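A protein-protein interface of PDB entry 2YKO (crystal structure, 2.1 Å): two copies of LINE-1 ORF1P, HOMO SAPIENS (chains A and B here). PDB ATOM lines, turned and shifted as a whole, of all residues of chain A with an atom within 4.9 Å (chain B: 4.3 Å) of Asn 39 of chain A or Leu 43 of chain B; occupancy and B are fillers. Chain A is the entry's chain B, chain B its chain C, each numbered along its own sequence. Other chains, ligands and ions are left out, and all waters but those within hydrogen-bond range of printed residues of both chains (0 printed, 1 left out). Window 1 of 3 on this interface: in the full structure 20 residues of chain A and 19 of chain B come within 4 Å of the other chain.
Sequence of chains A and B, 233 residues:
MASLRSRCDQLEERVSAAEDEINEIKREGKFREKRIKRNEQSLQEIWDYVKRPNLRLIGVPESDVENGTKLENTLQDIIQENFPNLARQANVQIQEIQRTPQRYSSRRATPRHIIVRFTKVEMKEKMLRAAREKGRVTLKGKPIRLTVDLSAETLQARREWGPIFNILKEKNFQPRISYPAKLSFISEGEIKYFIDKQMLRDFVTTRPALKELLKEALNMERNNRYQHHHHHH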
ATOM      1  N   ARG A  35     -15.349 -32.314   1.699  1.00  0.00           N
ATOM      2  CA  ARG A  35     -15.991 -31.548   2.759  1.00  0.00           C
ATOM      3  C   ARG A  35     -16.302 -30.115   2.316  1.00  0.00           C
ATOM      4  O   ARG A  35     -17.324 -29.536   2.735  1.00  0.00           O
ATOM      5  CB  ARG A  35     -15.129 -31.583   4.015  1.00  0.00           C
ATOM      6  CG  ARG A  35     -15.033 -32.990   4.571  1.00  0.00           C
ATOM      7  CD  ARG A  35     -13.844 -33.118   5.467  1.00  0.00           C
ATOM      8  NE  ARG A  35     -13.925 -32.232   6.609  1.00  0.00           N
ATOM      9  CZ  ARG A  35     -12.905 -31.990   7.428  1.00  0.00           C
ATOM     10  NH1 ARG A  35     -11.722 -32.562   7.202  1.00  0.00           N
ATOM     11  NH2 ARG A  35     -13.067 -31.172   8.463  1.00  0.00           N
ATOM     12  N   ILE A  36     -15.474 -29.569   1.429  1.00  0.00           N
ATOM     13  CA  ILE A  36     -15.747 -28.260   0.844  1.00  0.00           C
ATOM     14  C   ILE A  36     -17.036 -28.388  -0.001  1.00  0.00           C
ATOM     15  O   ILE A  36     -17.925 -27.561   0.084  1.00  0.00           O
ATOM     16  CB  ILE A  36     -14.582 -27.743  -0.028  1.00  0.00           C
ATOM     17  CG1 ILE A  36     -13.330 -27.451   0.824  1.00  0.00           C
ATOM     18  CG2 ILE A  36     -14.965 -26.465  -0.845  1.00  0.00           C
ATOM     19  CD1 ILE A  36     -12.133 -27.000  -0.016  1.00  0.00           C
ATOM     20  N   LYS A  37     -17.114 -29.437  -0.811  1.00  0.00           N
ATOM     21  CA  LYS A  37     -18.292 -29.695  -1.614  1.00  0.00           C
ATOM     22  C   LYS A  37     -19.548 -29.836  -0.754  1.00  0.00           C
ATOM     23  O   LYS A  37     -20.573 -29.292  -1.109  1.00  0.00           O
ATOM     24  CB  LYS A  37     -18.157 -30.993  -2.389  1.00  0.00           C
ATOM     25  CG  LYS A  37     -17.722 -30.830  -3.823  1.00  0.00           C
ATOM     26  CD  LYS A  37     -18.870 -31.045  -4.800  1.00  0.00           C
ATOM     27  CE  LYS A  37     -18.344 -31.250  -6.217  1.00  0.00           C
ATOM     28  NZ  LYS A  37     -19.422 -31.551  -7.217  1.00  0.00           N
ATOM     29  N   ARG A  38     -19.454 -30.630   0.310  1.00  0.00           N
ATOM     30  CA  ARG A  38     -20.513 -30.822   1.299  1.00  0.00           C
ATOM     31  C   ARG A  38     -20.980 -29.457   1.833  1.00  0.00           C
ATOM     32  O   ARG A  38     -22.158 -29.175   1.895  1.00  0.00           O
ATOM     33  CB  ARG A  38     -19.928 -31.608   2.467  1.00  0.00           C
ATOM     34  CG  ARG A  38     -20.651 -32.871   2.919  1.00  0.00           C
ATOM     35  CD  ARG A  38     -19.663 -33.963   3.480  1.00  0.00           C
ATOM     36  NE  ARG A  38     -19.104 -33.660   4.808  1.00  0.00           N
ATOM     37  CZ  ARG A  38     -18.236 -34.434   5.472  1.00  0.00           C
ATOM     38  NH1 ARG A  38     -17.789 -35.581   4.941  1.00  0.00           N
ATOM     39  NH2 ARG A  38     -17.804 -34.058   6.685  1.00  0.00           N
ATOM     40  N   ASN A  39     -20.032 -28.631   2.235  1.00  0.00           N
ATOM     41  CA  ASN A  39     -20.325 -27.313   2.778  1.00  0.00           C
ATOM     42  C   ASN A  39     -20.996 -26.453   1.710  1.00  0.00           C
ATOM     43  O   ASN A  39     -21.929 -25.723   2.027  1.00  0.00           O
ATOM     44  CB  ASN A  39     -19.069 -26.620   3.292  1.00  0.00           C
ATOM     45  CG  ASN A  39     -18.561 -27.212   4.610  1.00  0.00           C
ATOM     46  OD1 ASN A  39     -19.229 -28.027   5.216  1.00  0.00           O
ATOM     47  ND2 ASN A  39     -17.371 -26.804   5.036  1.00  0.00           N
ATOM     48  N   GLU A  40     -20.538 -26.531   0.454  1.00  0.00           N
ATOM     49  CA  GLU A  40     -21.110 -25.671  -0.599  1.00  0.00           C
ATOM     50  C   GLU A  40     -22.566 -26.096  -0.760  1.00  0.00           C
ATOM     51  O   GLU A  40     -23.471 -25.267  -0.917  1.00  0.00           O
ATOM     52  CB  GLU A  40     -20.362 -25.793  -1.947  1.00  0.00           C
ATOM     53  CG  GLU A  40     -18.975 -25.130  -1.927  1.00  0.00           C
ATOM     54  CD  GLU A  40     -18.109 -25.509  -3.128  1.00  0.00           C
ATOM     55  OE1 GLU A  40     -18.245 -26.638  -3.661  1.00  0.00           O
ATOM     56  OE2 GLU A  40     -17.285 -24.666  -3.544  1.00  0.00           O
ATOM     57  N   GLN A  41     -22.810 -27.399  -0.710  1.00  0.00           N
ATOM     58  CA  GLN A  41     -24.167 -27.865  -0.983  1.00  0.00           C
ATOM     59  C   GLN A  41     -25.094 -27.486   0.170  1.00  0.00           C
ATOM     60  O   GLN A  41     -26.244 -27.071  -0.038  1.00  0.00           O
ATOM     61  CB  GLN A  41     -24.226 -29.371  -1.258  1.00  0.00           C
ATOM     62  CG  GLN A  41     -25.178 -29.719  -2.434  1.00  0.00           C
ATOM     63  CD  GLN A  41     -24.678 -29.249  -3.821  1.00  0.00           C
ATOM     64  OE1 GLN A  41     -23.513 -28.851  -3.986  1.00  0.00           O
ATOM     65  NE2 GLN A  41     -25.572 -29.297  -4.822  1.00  0.00           N
ATOM     66  N   SER A  42     -24.571 -27.602   1.382  1.00  0.00           N
ATOM     67  CA  SER A  42     -25.307 -27.290   2.586  1.00  0.00           C
ATOM     68  C   SER A  42     -25.624 -25.774   2.659  1.00  0.00           C
ATOM     69  O   SER A  42     -26.667 -25.371   3.193  1.00  0.00           O
ATOM     70  CB  SER A  42     -24.512 -27.795   3.801  1.00  0.00           C
ATOM     71  OG  SER A  42     -25.151 -27.426   4.999  1.00  0.00           O
ATOM     72  N   LEU A  43     -24.735 -24.947   2.107  1.00  0.00           N
ATOM     73  CA  LEU A  43     -24.963 -23.509   2.010  1.00  0.00           C
ATOM     74  C   LEU A  43     -26.072 -23.232   1.012  1.00  0.00           C
ATOM     75  O   LEU A  43     -26.857 -22.323   1.224  1.00  0.00           O
ATOM     76  CB  LEU A  43     -23.710 -22.769   1.554  1.00  0.00           C
ATOM     77  CG  LEU A  43     -22.779 -22.435   2.728  1.00  0.00           C
ATOM     78  CD1 LEU A  43     -21.404 -21.956   2.230  1.00  0.00           C
ATOM     79  CD2 LEU A  43     -23.452 -21.393   3.603  1.00  0.00           C
ATOM     80  N   ILE A  46     -29.419 -24.123   2.890  1.00  0.00           N
ATOM     81  CA  ILE A  46     -29.861 -23.210   3.952  1.00  0.00           C
ATOM     82  C   ILE A  46     -30.295 -21.843   3.376  1.00  0.00           C
ATOM     83  O   ILE A  46     -31.236 -21.232   3.847  1.00  0.00           O
ATOM     84  CB  ILE A  46     -28.791 -23.045   5.074  1.00  0.00           C
ATOM     85  CG1 ILE A  46     -29.314 -22.201   6.241  1.00  0.00           C
ATOM     86  CG2 ILE A  46     -27.568 -22.325   4.566  1.00  0.00           C
ATOM     87  CD1 ILE A  46     -30.325 -22.822   7.031  1.00  0.00           C
ATOM     88  N   ILE B  36     -12.161 -25.311   7.131  1.00  0.00           N
ATOM     89  CA  ILE B  36     -13.234 -26.161   6.622  1.00  0.00           C
ATOM     90  C   ILE B  36     -14.038 -26.680   7.818  1.00  0.00           C
ATOM     91  O   ILE B  36     -15.267 -26.704   7.784  1.00  0.00           O
ATOM     92  CB  ILE B  36     -12.699 -27.367   5.840  1.00  0.00           C
ATOM     93  CG1 ILE B  36     -11.996 -26.916   4.546  1.00  0.00           C
ATOM     94  CG2 ILE B  36     -13.859 -28.379   5.496  1.00  0.00           C
ATOM     95  CD1 ILE B  36     -11.309 -28.105   3.797  1.00  0.00           C
ATOM     96  N   ASN B  39     -16.214 -23.960   9.181  1.00  0.00           N
ATOM     97  CA  ASN B  39     -17.370 -23.746   8.350  1.00  0.00           C
ATOM     98  C   ASN B  39     -18.409 -24.851   8.618  1.00  0.00           C
ATOM     99  O   ASN B  39     -19.595 -24.591   8.616  1.00  0.00           O
ATOM    100  CB  ASN B  39     -16.978 -23.723   6.871  1.00  0.00           C
ATOM    101  CG  ASN B  39     -16.267 -22.432   6.490  1.00  0.00           C
ATOM    102  OD1 ASN B  39     -16.247 -21.489   7.272  1.00  0.00           O
ATOM    103  ND2 ASN B  39     -15.683 -22.391   5.294  1.00  0.00           N
ATOM    104  N   GLU B  40     -17.957 -26.082   8.849  1.00  0.00           N
ATOM    105  CA  GLU B  40     -18.885 -27.184   9.090  1.00  0.00           C
ATOM    106  C   GLU B  40     -19.651 -26.952  10.396  1.00  0.00           C
ATOM    107  O   GLU B  40     -20.835 -27.208  10.467  1.00  0.00           O
ATOM    108  CB  GLU B  40     -18.116 -28.537   9.196  1.00  0.00           C
ATOM    109  CG  GLU B  40     -17.651 -29.113   7.826  1.00  0.00           C
ATOM    110  CD  GLU B  40     -16.669 -30.312   7.971  1.00  0.00           C
ATOM    111  OE1 GLU B  40     -16.120 -30.530   9.085  1.00  0.00           O
ATOM    112  OE2 GLU B  40     -16.461 -31.043   6.968  1.00  0.00           O
ATOM    113  N   GLN B  41     -18.929 -26.504  11.420  1.00  0.00           N
ATOM    114  CA  GLN B  41     -19.494 -26.268  12.731  1.00  0.00           C
ATOM    115  C   GLN B  41     -20.505 -25.089  12.701  1.00  0.00           C
ATOM    116  O   GLN B  41     -21.605 -25.152  13.291  1.00  0.00           O
ATOM    117  CB  GLN B  41     -18.374 -25.976  13.705  1.00  0.00           C
ATOM    118  CG  GLN B  41     -18.840 -25.390  14.999  1.00  0.00           C
ATOM    119  CD  GLN B  41     -17.722 -25.371  16.018  1.00  0.00           C
ATOM    120  OE1 GLN B  41     -16.703 -26.033  15.834  1.00  0.00           O
ATOM    121  NE2 GLN B  41     -17.894 -24.593  17.087  1.00  0.00           N
ATOM    122  N   SER B  42     -20.127 -24.036  11.991  1.00  0.00           N
ATOM    123  CA  SER B  42     -20.975 -22.881  11.827  1.00  0.00           C
ATOM    124  C   SER B  42     -22.260 -23.197  11.051  1.00  0.00           C
ATOM    125  O   SER B  42     -23.308 -22.611  11.343  1.00  0.00           O
ATOM    126  CB  SER B  42     -20.200 -21.750  11.149  1.00  0.00           C
ATOM    127  OG  SER B  42     -21.075 -20.658  10.953  1.00  0.00           O
ATOM    128  N   LEU B  43     -22.197 -24.111  10.067  1.00  0.00           N
ATOM    129  CA  LEU B  43     -23.403 -24.585   9.381  1.00  0.00           C
ATOM    130  C   LEU B  43     -24.360 -25.381  10.328  1.00  0.00           C
ATOM    131  O   LEU B  43     -25.586 -25.196  10.286  1.00  0.00           O
ATOM    132  CB  LEU B  43     -23.047 -25.454   8.174  1.00  0.00           C
ATOM    133  CG  LEU B  43     -22.689 -24.709   6.878  1.00  0.00           C
ATOM    134  CD1 LEU B  43     -21.896 -25.637   5.978  1.00  0.00           C
ATOM    135  CD2 LEU B  43     -23.950 -24.185   6.179  1.00  0.00           C
ATOM    136  N   GLN B  44     -23.803 -26.267  11.139  1.00  0.00           N
ATOM    137  CA  GLN B  44     -24.589 -26.984  12.159  1.00  0.00           C
ATOM    138  C   GLN B  44     -25.320 -25.952  13.062  1.00  0.00           C
ATOM    139  O   GLN B  44     -26.535 -26.070  13.330  1.00  0.00           O
ATOM    140  CB  GLN B  44     -23.645 -27.908  12.967  1.00  0.00           C
ATOM    141  CG  GLN B  44     -24.252 -28.695  14.122  1.00  0.00           C
ATOM    142  CD  GLN B  44     -23.320 -29.871  14.589  1.00  0.00           C
ATOM    143  OE1 GLN B  44     -22.225 -30.061  14.047  1.00  0.00           O
ATOM    144  NE2 GLN B  44     -23.760 -30.631  15.581  1.00  0.00           N
ATOM    145  N   GLU B  45     -24.587 -24.939  13.529  1.00  0.00           N
ATOM    146  CA  GLU B  45     -25.159 -23.901  14.406  1.00  0.00           C
ATOM    147  C   GLU B  45     -26.288 -23.072  13.789  1.00  0.00           C
ATOM    148  O   GLU B  45     -27.290 -22.788  14.457  1.00  0.00           O
ATOM    149  CB  GLU B  45     -24.076 -22.982  14.978  1.00  0.00           C
ATOM    150  CG  GLU B  45     -23.166 -23.750  15.932  1.00  0.00           C
ATOM    151  CD  GLU B  45     -22.058 -22.873  16.547  1.00  0.00           C
ATOM    152  OE1 GLU B  45     -22.070 -21.638  16.297  1.00  0.00           O
ATOM    153  OE2 GLU B  45     -21.190 -23.425  17.276  1.00  0.00           O
ATOM    154  N   ILE B  46     -26.147 -22.699  12.533  1.00  0.00           N
ATOM    155  CA  ILE B  46     -27.124 -21.812  11.942  1.00  0.00           C
ATOM    156  C   ILE B  46     -28.367 -22.627  11.565  1.00  0.00           C
ATOM    157  O   ILE B  46     -29.462 -22.148  11.708  1.00  0.00           O
ATOM    158  CB  ILE B  46     -26.596 -21.022  10.739  1.00  0.00           C
ATOM    159  CG1 ILE B  46     -27.633 -20.004  10.292  1.00  0.00           C
ATOM    160  CG2 ILE B  46     -26.361 -21.911   9.556  1.00  0.00           C
ATOM    161  CD1 ILE B  46     -27.018 -18.920   9.469  1.00  0.00           C
ATOM    162  N   TRP B  47     -28.195 -23.885  11.182  1.00  0.00           N
ATOM    163  CA  TRP B  47     -29.341 -24.804  11.007  1.00  0.00           C
ATOM    164  C   TRP B  47     -30.114 -24.943  12.347  1.00  0.00           C
ATOM    165  O   TRP B  47     -31.364 -24.834  12.393  1.00  0.00           O
ATOM    166  CB  TRP B  47     -28.867 -26.180  10.461  1.00  0.00           C
ATOM    167  CG  TRP B  47     -28.895 -26.281   8.959  1.00  0.00           C
ATOM    168  CD1 TRP B  47     -27.834 -26.523   8.139  1.00  0.00           C
ATOM    169  CD2 TRP B  47     -30.058 -26.151   8.086  1.00  0.00           C
ATOM    170  NE1 TRP B  47     -28.248 -26.545   6.818  1.00  0.00           N
ATOM    171  CE2 TRP B  47     -29.603 -26.322   6.760  1.00  0.00           C
ATOM    172  CE3 TRP B  47     -31.422 -25.898   8.305  1.00  0.00           C
ATOM    173  CZ2 TRP B  47     -30.459 -26.264   5.656  1.00  0.00           C
ATOM    174  CZ3 TRP B  47     -32.284 -25.822   7.204  1.00  0.00           C
ATOM    175  CH2 TRP B  47     -31.801 -26.014   5.901  1.00  0.00           C
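NE of Arg 35 of chain A is in salt-bridge range of OE2 of Glu 40 of chain B. OE2 of Glu 40 of chain B lies within salt-bridge range of NH2 of Arg 38 of chain A, 3.3 Å away. The side-chain amide nitrogen (ND2) of Asn 39 of chain A is in hydrogen-bond range of the backbone carbonyl oxygen (O) of Ile 36 of chain B (3.5 Å).
The backbone carbonyl oxygen (O) of Arg 35 of chain A sits close to the side-chain amide oxygen (OD1) of Asn 39 of chain A, 3.5 Å away.
CB of Arg 35 of chain A touches CG2 of Ile 36 of chain B, at 3.8 Å. CD1 of Ile 36 of chain B touches CG1 of Ile 36 of chain A (3.7 Å). CB of Asn 39 of chain B touches ND2 of Asn 39 of chain A, 3.6 Å away. Glu 40 of chain B touches Asn 39 of chain A. Asn 39 of chain A touches Leu 43 of chain B (OD1 to CD1, 3.7 Å). Ser 42 of chain A touches Leu 43 of chain B. Trp 47 of chain B touches Ser 42 of chain A. Leu 43 of chain B touches Leu 43 of chain A. Ile 46 of chain A touches Trp 47 of chain B.
Of chain B, only Ile 36 (3.5 Å), Asn 39 (3.6 Å), Glu 40 (3.2 Å) and Leu 43 (3.7 Å) come within 4 Å of Asn 39 of chain A. Of the printed residues of chain A, Ile 36 of chain B touches Arg 35, Ile 36 and Asn 39. Printed residues of chain A within 4 Å of Asn 39 of chain B: Asn 39 (3.6 Å). Of the printed residues of chain A, Glu 40 of chain B touches Arg 35, Arg 38 and Asn 39. Of the printed residues of chain A, Leu 43 of chain B touches Asn 39, Ser 42 and Leu 43. The nearest printed residue of chain B that does not touch Asn 39 of chain A is Gln 41 of chain B (6.4 Å). The nearest residue of chain A that does not touch Leu 43 of chain B is Ile 46 of chain A (4.4 Å). The nearest printed residue of chain B that does not touch Arg 38 of chain A is Leu 43 of chain B (5.4 Å).
Hydrophobic or aromatic side chains of chain A that line the printed part of chain B: Ile 36, Leu 43 and Ile 46. Hydrophobic or aromatic side chains of chain B within 4 Å of the printed part of chain A: Ile 36, Leu 43 and Trp 47. Among the printed residues, 12 pairs touch across the chains. Among the printed residues, Asp or Glu carboxylates within 4 Å of a Lys or Arg side-chain nitrogen of the other chain: Arg 35 of chain A with Glu 40 of chain B (2.8 Å) and Arg 38 of chain A with Glu 40 of chain B (3.3 Å).
Asn 39 of chain A touches Ile 36 of chain B, but with the chains exchanged Ile 36 of chain A does not touch Asn 39 of chain B (7.1 Å). Asn 39 of chain B touches its own counterpart, Asn 39 of chain A. Ser 42 of chain A touches Leu 43 of chain B, but with the chains exchanged Leu 43 of chain A does not touch Ser 42 of chain B (7.8 Å). Leu 43 of chain B touches its own counterpart, Leu 43 of chain A. Of the 12 pairs that touch across the chains among the printed residues, 3 have their exchanged pair printed and touching as well.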
